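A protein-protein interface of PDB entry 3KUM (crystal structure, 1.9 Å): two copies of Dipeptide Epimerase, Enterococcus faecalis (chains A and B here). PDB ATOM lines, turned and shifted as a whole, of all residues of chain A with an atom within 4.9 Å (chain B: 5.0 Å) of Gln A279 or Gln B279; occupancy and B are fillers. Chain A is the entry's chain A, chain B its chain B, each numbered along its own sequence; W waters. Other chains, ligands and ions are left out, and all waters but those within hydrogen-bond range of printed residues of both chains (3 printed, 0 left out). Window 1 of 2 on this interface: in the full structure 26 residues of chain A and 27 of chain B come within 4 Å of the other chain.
The side-chain amino group (NZ) of Lys B276 lies within salt-bridge range of the side-chain carboxylate (OE1) of Glu A282.
The side-chain amino group of Lys A276 lies within salt-bridge range of the side-chain carboxylate of Glu B282.
OG1 of Thr A283 is in hydrogen-bond range of O of Gln A279.
The side-chain amide oxygen of Gln A311 sits close to the side-chain amide oxygen of Gln A279.
The side-chain hydroxyl (OG1) of Thr B283 sits at hydrogen-bond distance from the backbone carbonyl oxygen (O) of Gln B279 (2.7 Å).
The side-chain amide oxygen (OE1) of Gln A279 lies close to the side-chain carboxylate (OE1) of Glu A282 (3.4 Å).
Among the printed residues, merely in contact across the chains: Lys A276 with Gln B279 (3.8 Å), Gln A279 with Lys B276 (3.5 Å), Gln A279 with Gln B279 (2.9 Å), Ile A280 with Thr B283 (3.8 Å) and Thr A283 with Ile B280 (3.8 Å).
Of chain B, only Lys B276 and Gln B279 come within 4 Å of Gln A279.
Gln B279 touches two residues of chain A.
Of the printed residues of chain A, Glu B282 touches Lys A276.
Printed residues of chain B within 4 Å of Lys A276: Gln B279 and Glu B282.
Of the printed residues of chain A, Ile B280 touches Thr A283.
The nearest printed residue of chain B that does not touch Gln A279 is His B272 (4.8 Å).
The nearest residue of chain A that does not touch Gln B279 is Leu A275 (4.2 Å).
Of the 11 printed residues of chain B, 5 touch a printed residue of chain A.
Hydrophobic or aromatic side chains of chain B that line the printed part of chain A: Ile B280.
Of the 11 printed residues of chain A, 5 touch a printed residue of chain B.
Along chain A the printed residues that touch a printed residue of chain B span positions 276 to 283.
Among the printed residues, Asp or Glu carboxylates within 4 Å of a Lys or Arg side-chain nitrogen of the other chain: Lys A276 with Glu B282 (3.6 Å) and Glu A282 with Lys B276 (3.7 Å).
Lys A276 touches Gln B279, and with the chains exchanged Gln A279 touches Lys B276.
Lys A276 touches Glu B282, and with the chains exchanged Glu A282 touches Lys B276.
Gln A279 touches its own counterpart, Gln B279.
Ile A280 touches Thr B283, and with the chains exchanged Thr A283 touches Ile B280.
Positions printed for both chains: 272, 275, 276, 277, 278, 279, 280, 281, 282, 283 and 311.
Water W3 lies within hydrogen-bond range of NE2 of Gln A279 (2.7 Å) and O of His B272 (2.8 Å).
Water W2 lies within hydrogen-bond range of the side-chain amide nitrogen (NE2) of Gln B279 and the backbone carbonyl oxygen (O) of His A272.
Water W1 bridges OG1 of Thr A283 (2.9 Å) and NZ of Lys B276 (3.0 Å).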
ATOM      1  N   HIS A 272       1.592  30.320   0.430  1.00  0.00           N
ATOM      2  CA  HIS A 272       1.555  29.255   1.437  1.00  0.00           C
ATOM      3  C   HIS A 272       2.965  28.896   1.935  1.00  0.00           C
ATOM      4  O   HIS A 272       3.206  28.727   3.133  1.00  0.00           O
ATOM      5  CB  HIS A 272       0.869  28.023   0.841  1.00  0.00           C
ATOM      6  CG  HIS A 272       0.632  26.922   1.826  1.00  0.00           C
ATOM      7  ND1 HIS A 272       1.446  25.811   1.915  1.00  0.00           N
ATOM      8  CD2 HIS A 272      -0.327  26.765   2.769  1.00  0.00           C
ATOM      9  CE1 HIS A 272       0.996  25.017   2.870  1.00  0.00           C
ATOM     10  NE2 HIS A 272      -0.080  25.572   3.404  1.00  0.00           N
ATOM     11  N   LEU A 275       4.855  31.975   3.707  1.00  0.00           N
ATOM     12  CA  LEU A 275       4.455  32.125   5.101  1.00  0.00           C
ATOM     13  C   LEU A 275       5.338  31.247   5.979  1.00  0.00           C
ATOM     14  O   LEU A 275       5.796  31.685   7.036  1.00  0.00           O
ATOM     15  CB  LEU A 275       2.975  31.755   5.271  1.00  0.00           C
ATOM     16  CG  LEU A 275       1.966  32.797   4.770  1.00  0.00           C
ATOM     17  CD1 LEU A 275       0.542  32.230   4.858  1.00  0.00           C
ATOM     18  CD2 LEU A 275       2.084  34.068   5.607  1.00  0.00           C
ATOM     19  N   LYS A 276       5.599  30.018   5.531  1.00  0.00           N
ATOM     20  CA  LYS A 276       6.444  29.107   6.287  1.00  0.00           C
ATOM     21  C   LYS A 276       7.831  29.708   6.464  1.00  0.00           C
ATOM     22  O   LYS A 276       8.353  29.755   7.572  1.00  0.00           O
ATOM     23  CB  LYS A 276       6.582  27.759   5.578  1.00  0.00           C
ATOM     24  CG  LYS A 276       5.313  26.929   5.501  1.00  0.00           C
ATOM     25  CD  LYS A 276       5.641  25.612   4.803  1.00  0.00           C
ATOM     26  CE  LYS A 276       4.401  24.784   4.491  1.00  0.00           C
ATOM     27  NZ  LYS A 276       4.776  23.609   3.637  1.00  0.00           N
ATOM     28  N   ILE A 277       8.433  30.151   5.364  1.00  0.00           N
ATOM     29  CA  ILE A 277       9.762  30.747   5.422  1.00  0.00           C
ATOM     30  C   ILE A 277       9.831  31.892   6.431  1.00  0.00           C
ATOM     31  O   ILE A 277      10.701  31.917   7.298  1.00  0.00           O
ATOM     32  CB  ILE A 277      10.195  31.290   4.051  1.00  0.00           C
ATOM     33  CG1 ILE A 277      10.359  30.139   3.056  1.00  0.00           C
ATOM     34  CG2 ILE A 277      11.505  32.063   4.199  1.00  0.00           C
ATOM     35  CD1 ILE A 277      10.367  30.577   1.590  1.00  0.00           C
ATOM     36  N   ASN A 278       8.917  32.847   6.302  1.00  0.00           N
ATOM     37  CA  ASN A 278       8.892  33.984   7.202  1.00  0.00           C
ATOM     38  C   ASN A 278       8.723  33.549   8.664  1.00  0.00           C
ATOM     39  O   ASN A 278       9.359  34.114   9.556  1.00  0.00           O
ATOM     40  CB  ASN A 278       7.771  34.956   6.801  1.00  0.00           C
ATOM     41  CG  ASN A 278       7.794  36.237   7.617  1.00  0.00           C
ATOM     42  OD1 ASN A 278       8.818  36.912   7.703  1.00  0.00           O
ATOM     43  ND2 ASN A 278       6.663  36.578   8.218  1.00  0.00           N
ATOM     44  N   GLN A 279       7.891  32.538   8.905  1.00  0.00           N
ATOM     45  CA  GLN A 279       7.660  32.053  10.268  1.00  0.00           C
ATOM     46  C   GLN A 279       8.909  31.421  10.858  1.00  0.00           C
ATOM     47  O   GLN A 279       9.199  31.577  12.043  1.00  0.00           O
ATOM     48  CB  GLN A 279       6.536  31.016  10.299  1.00  0.00           C
ATOM     49  CG  GLN A 279       5.210  31.516   9.798  1.00  0.00           C
ATOM     50  CD  GLN A 279       4.768  32.755  10.516  1.00  0.00           C
ATOM     51  OE1 GLN A 279       5.475  33.767  10.519  1.00  0.00           O
ATOM     52  NE2 GLN A 279       3.590  32.696  11.136  1.00  0.00           N
ATOM     53  N   ILE A 280       9.638  30.686  10.023  1.00  0.00           N
ATOM     54  CA  ILE A 280      10.857  30.039  10.458  1.00  0.00           C
ATOM     55  C   ILE A 280      11.897  31.109  10.787  1.00  0.00           C
ATOM     56  O   ILE A 280      12.581  31.026  11.803  1.00  0.00           O
ATOM     57  CB  ILE A 280      11.399  29.101   9.349  1.00  0.00           C
ATOM     58  CG1 ILE A 280      10.443  27.917   9.174  1.00  0.00           C
ATOM     59  CG2 ILE A 280      12.808  28.611   9.706  1.00  0.00           C
ATOM     60  CD1 ILE A 280      10.699  27.108   7.933  1.00  0.00           C
ATOM     61  N   CYS A 281      11.991  32.120   9.930  1.00  0.00           N
ATOM     62  CA  CYS A 281      12.945  33.213  10.109  1.00  0.00           C
ATOM     63  C   CYS A 281      12.627  34.067  11.344  1.00  0.00           C
ATOM     64  O   CYS A 281      13.513  34.398  12.130  1.00  0.00           O
ATOM     65  CB  CYS A 281      12.962  34.102   8.862  1.00  0.00           C
ATOM     66  SG  CYS A 281      13.737  33.344   7.369  1.00  0.00           S
ATOM     67  N   GLU A 282      11.367  34.441  11.501  1.00  0.00           N
ATOM     68  CA  GLU A 282      10.962  35.244  12.652  1.00  0.00           C
ATOM     69  C   GLU A 282      11.304  34.493  13.946  1.00  0.00           C
ATOM     70  O   GLU A 282      11.884  35.054  14.875  1.00  0.00           O
ATOM     71  CB  GLU A 282       9.465  35.534  12.559  1.00  0.00           C
ATOM     72  CG  GLU A 282       8.867  36.263  13.747  1.00  0.00           C
ATOM     73  CD  GLU A 282       7.430  36.685  13.494  1.00  0.00           C
ATOM     74  OE1 GLU A 282       6.659  35.864  12.958  1.00  0.00           O
ATOM     75  OE2 GLU A 282       7.070  37.831  13.838  1.00  0.00           O
ATOM     76  N   THR A 283      10.951  33.215  13.996  1.00  0.00           N
ATOM     77  CA  THR A 283      11.233  32.396  15.167  1.00  0.00           C
ATOM     78  C   THR A 283      12.734  32.388  15.490  1.00  0.00           C
ATOM     79  O   THR A 283      13.118  32.397  16.658  1.00  0.00           O
ATOM     80  CB  THR A 283      10.726  30.964  14.942  1.00  0.00           C
ATOM     81  OG1 THR A 283       9.302  31.002  14.747  1.00  0.00           O
ATOM     82  CG2 THR A 283      11.062  30.073  16.124  1.00  0.00           C
ATOM     83  N   GLN A 311       2.548  40.681   7.070  1.00  0.00           N
ATOM     84  CA  GLN A 311       3.505  40.082   7.994  1.00  0.00           C
ATOM     85  C   GLN A 311       4.534  41.038   8.594  1.00  0.00           C
ATOM     86  O   GLN A 311       5.329  41.656   7.881  1.00  0.00           O
ATOM     87  CB  GLN A 311       4.218  38.935   7.285  1.00  0.00           C
ATOM     88  CG  GLN A 311       3.284  37.777   6.958  1.00  0.00           C
ATOM     89  CD  GLN A 311       3.046  36.902   8.161  1.00  0.00           C
ATOM     90  OE1 GLN A 311       3.979  36.292   8.674  1.00  0.00           O
ATOM     91  NE2 GLN A 311       1.805  36.834   8.621  1.00  0.00           N
ATOM     92  N   HIS B 272      -2.261  31.370  16.374  1.00  0.00           N
ATOM     93  CA  HIS B 272      -1.194  32.047  15.648  1.00  0.00           C
ATOM     94  C   HIS B 272       0.172  31.396  15.873  1.00  0.00           C
ATOM     95  O   HIS B 272       0.925  31.181  14.926  1.00  0.00           O
ATOM     96  CB  HIS B 272      -1.150  33.522  16.056  1.00  0.00           C
ATOM     97  CG  HIS B 272      -0.215  34.358  15.233  1.00  0.00           C
ATOM     98  ND1 HIS B 272       0.988  34.823  15.715  1.00  0.00           N
ATOM     99  CD2 HIS B 272      -0.329  34.846  13.974  1.00  0.00           C
ATOM    100  CE1 HIS B 272       1.573  35.568  14.794  1.00  0.00           C
ATOM    101  NE2 HIS B 272       0.793  35.597  13.728  1.00  0.00           N
ATOM    102  N   LEU B 275       0.347  27.555  14.634  1.00  0.00           N
ATOM    103  CA  LEU B 275       0.590  27.427  13.204  1.00  0.00           C
ATOM    104  C   LEU B 275       2.087  27.468  12.915  1.00  0.00           C
ATOM    105  O   LEU B 275       2.574  26.727  12.055  1.00  0.00           O
ATOM    106  CB  LEU B 275      -0.119  28.544  12.425  1.00  0.00           C
ATOM    107  CG  LEU B 275      -1.634  28.401  12.261  1.00  0.00           C
ATOM    108  CD1 LEU B 275      -2.232  29.740  11.878  1.00  0.00           C
ATOM    109  CD2 LEU B 275      -1.945  27.316  11.208  1.00  0.00           C
ATOM    110  N   LYS B 276       2.809  28.337  13.621  1.00  0.00           N
ATOM    111  CA  LYS B 276       4.254  28.439  13.434  1.00  0.00           C
ATOM    112  C   LYS B 276       4.901  27.113  13.824  1.00  0.00           C
ATOM    113  O   LYS B 276       5.730  26.579  13.093  1.00  0.00           O
ATOM    114  CB  LYS B 276       4.857  29.527  14.319  1.00  0.00           C
ATOM    115  CG  LYS B 276       4.392  30.940  14.065  1.00  0.00           C
ATOM    116  CD  LYS B 276       5.179  31.879  14.990  1.00  0.00           C
ATOM    117  CE  LYS B 276       4.607  33.288  15.006  1.00  0.00           C
ATOM    118  NZ  LYS B 276       5.326  34.144  16.006  1.00  0.00           N
ATOM    119  N   ILE B 277       4.525  26.587  14.984  1.00  0.00           N
ATOM    120  CA  ILE B 277       5.088  25.321  15.443  1.00  0.00           C
ATOM    121  C   ILE B 277       4.873  24.205  14.426  1.00  0.00           C
ATOM    122  O   ILE B 277       5.801  23.447  14.114  1.00  0.00           O
ATOM    123  CB  ILE B 277       4.471  24.872  16.787  1.00  0.00           C
ATOM    124  CG1 ILE B 277       4.842  25.870  17.892  1.00  0.00           C
ATOM    125  CG2 ILE B 277       4.972  23.475  17.138  1.00  0.00           C
ATOM    126  CD1 ILE B 277       4.091  25.679  19.194  1.00  0.00           C
ATOM    127  N   ASN B 278       3.652  24.090  13.912  1.00  0.00           N
ATOM    128  CA  ASN B 278       3.363  23.039  12.941  1.00  0.00           C
ATOM    129  C   ASN B 278       4.135  23.199  11.616  1.00  0.00           C
ATOM    130  O   ASN B 278       4.591  22.214  11.035  1.00  0.00           O
ATOM    131  CB  ASN B 278       1.874  22.977  12.635  1.00  0.00           C
ATOM    132  CG  ASN B 278       1.541  21.845  11.690  1.00  0.00           C
ATOM    133  OD1 ASN B 278       1.879  20.691  11.957  1.00  0.00           O
ATOM    134  ND2 ASN B 278       0.895  22.166  10.577  1.00  0.00           N
ATOM    135  N   GLN B 279       4.272  24.434  11.152  1.00  0.00           N
ATOM    136  CA  GLN B 279       4.982  24.704   9.904  1.00  0.00           C
ATOM    137  C   GLN B 279       6.461  24.385  10.047  1.00  0.00           C
ATOM    138  O   GLN B 279       7.086  23.899   9.111  1.00  0.00           O
ATOM    139  CB  GLN B 279       4.835  26.169   9.501  1.00  0.00           C
ATOM    140  CG  GLN B 279       3.422  26.617   9.222  1.00  0.00           C
ATOM    141  CD  GLN B 279       3.354  28.108   8.917  1.00  0.00           C
ATOM    142  OE1 GLN B 279       3.894  28.940   9.661  1.00  0.00           O
ATOM    143  NE2 GLN B 279       2.693  28.453   7.825  1.00  0.00           N
ATOM    144  N   ILE B 280       7.020  24.692  11.214  1.00  0.00           N
ATOM    145  CA  ILE B 280       8.426  24.421  11.490  1.00  0.00           C
ATOM    146  C   ILE B 280       8.636  22.908  11.491  1.00  0.00           C
ATOM    147  O   ILE B 280       9.562  22.393  10.850  1.00  0.00           O
ATOM    148  CB  ILE B 280       8.834  25.013  12.864  1.00  0.00           C
ATOM    149  CG1 ILE B 280       8.953  26.536  12.755  1.00  0.00           C
ATOM    150  CG2 ILE B 280      10.146  24.403  13.360  1.00  0.00           C
ATOM    151  CD1 ILE B 280       9.119  27.226  14.113  1.00  0.00           C
ATOM    152  N   CYS B 281       7.760  22.201  12.195  1.00  0.00           N
ATOM    153  CA  CYS B 281       7.841  20.739  12.289  1.00  0.00           C
ATOM    154  C   CYS B 281       7.656  20.066  10.933  1.00  0.00           C
ATOM    155  O   CYS B 281       8.406  19.156  10.558  1.00  0.00           O
ATOM    156  CB  CYS B 281       6.781  20.218  13.263  1.00  0.00           C
ATOM    157  SG  CYS B 281       7.138  20.563  14.988  1.00  0.00           S
ATOM    158  N   GLU B 282       6.635  20.511  10.208  1.00  0.00           N
ATOM    159  CA  GLU B 282       6.334  19.977   8.891  1.00  0.00           C
ATOM    160  C   GLU B 282       7.574  20.118   8.013  1.00  0.00           C
ATOM    161  O   GLU B 282       7.977  19.175   7.327  1.00  0.00           O
ATOM    162  CB  GLU B 282       5.165  20.755   8.284  1.00  0.00           C
ATOM    163  CG  GLU B 282       4.719  20.307   6.912  1.00  0.00           C
ATOM    164  CD  GLU B 282       3.475  21.045   6.458  1.00  0.00           C
ATOM    165  OE1 GLU B 282       3.418  22.278   6.646  1.00  0.00           O
ATOM    166  OE2 GLU B 282       2.557  20.399   5.910  1.00  0.00           O
ATOM    167  N   THR B 283       8.183  21.301   8.050  1.00  0.00           N
ATOM    168  CA  THR B 283       9.375  21.565   7.251  1.00  0.00           C
ATOM    169  C   THR B 283      10.513  20.608   7.617  1.00  0.00           C
ATOM    170  O   THR B 283      11.271  20.176   6.750  1.00  0.00           O
ATOM    171  CB  THR B 283       9.831  23.027   7.437  1.00  0.00           C
ATOM    172  OG1 THR B 283       8.768  23.902   7.039  1.00  0.00           O
ATOM    173  CG2 THR B 283      11.075  23.323   6.586  1.00  0.00           C
ATOM    174  N   GLN B 311      -4.957  21.575   9.265  1.00  0.00           N
ATOM    175  CA  GLN B 311      -3.561  21.311   8.920  1.00  0.00           C
ATOM    176  C   GLN B 311      -3.212  19.854   8.706  1.00  0.00           C
ATOM    177  O   GLN B 311      -3.360  19.034   9.599  1.00  0.00           O
ATOM    178  CB  GLN B 311      -2.648  21.883  10.015  1.00  0.00           C
ATOM    179  CG  GLN B 311      -2.692  23.402  10.117  1.00  0.00           C
ATOM    180  CD  GLN B 311      -1.922  24.078   8.988  1.00  0.00           C
ATOM    181  OE1 GLN B 311      -0.707  23.932   8.886  1.00  0.00           O
ATOM    182  NE2 GLN B 311      -2.626  24.813   8.137  1.00  0.00           N
HETATM  183  O   HOH W   1       8.155  33.268  16.215  1.00  0.00           O
HETATM  184  O   HOH W   2       1.500  28.259   5.324  1.00  0.00           O
HETATM  185  O   HOH W   3       1.266  32.368  12.457  1.00  0.00           O
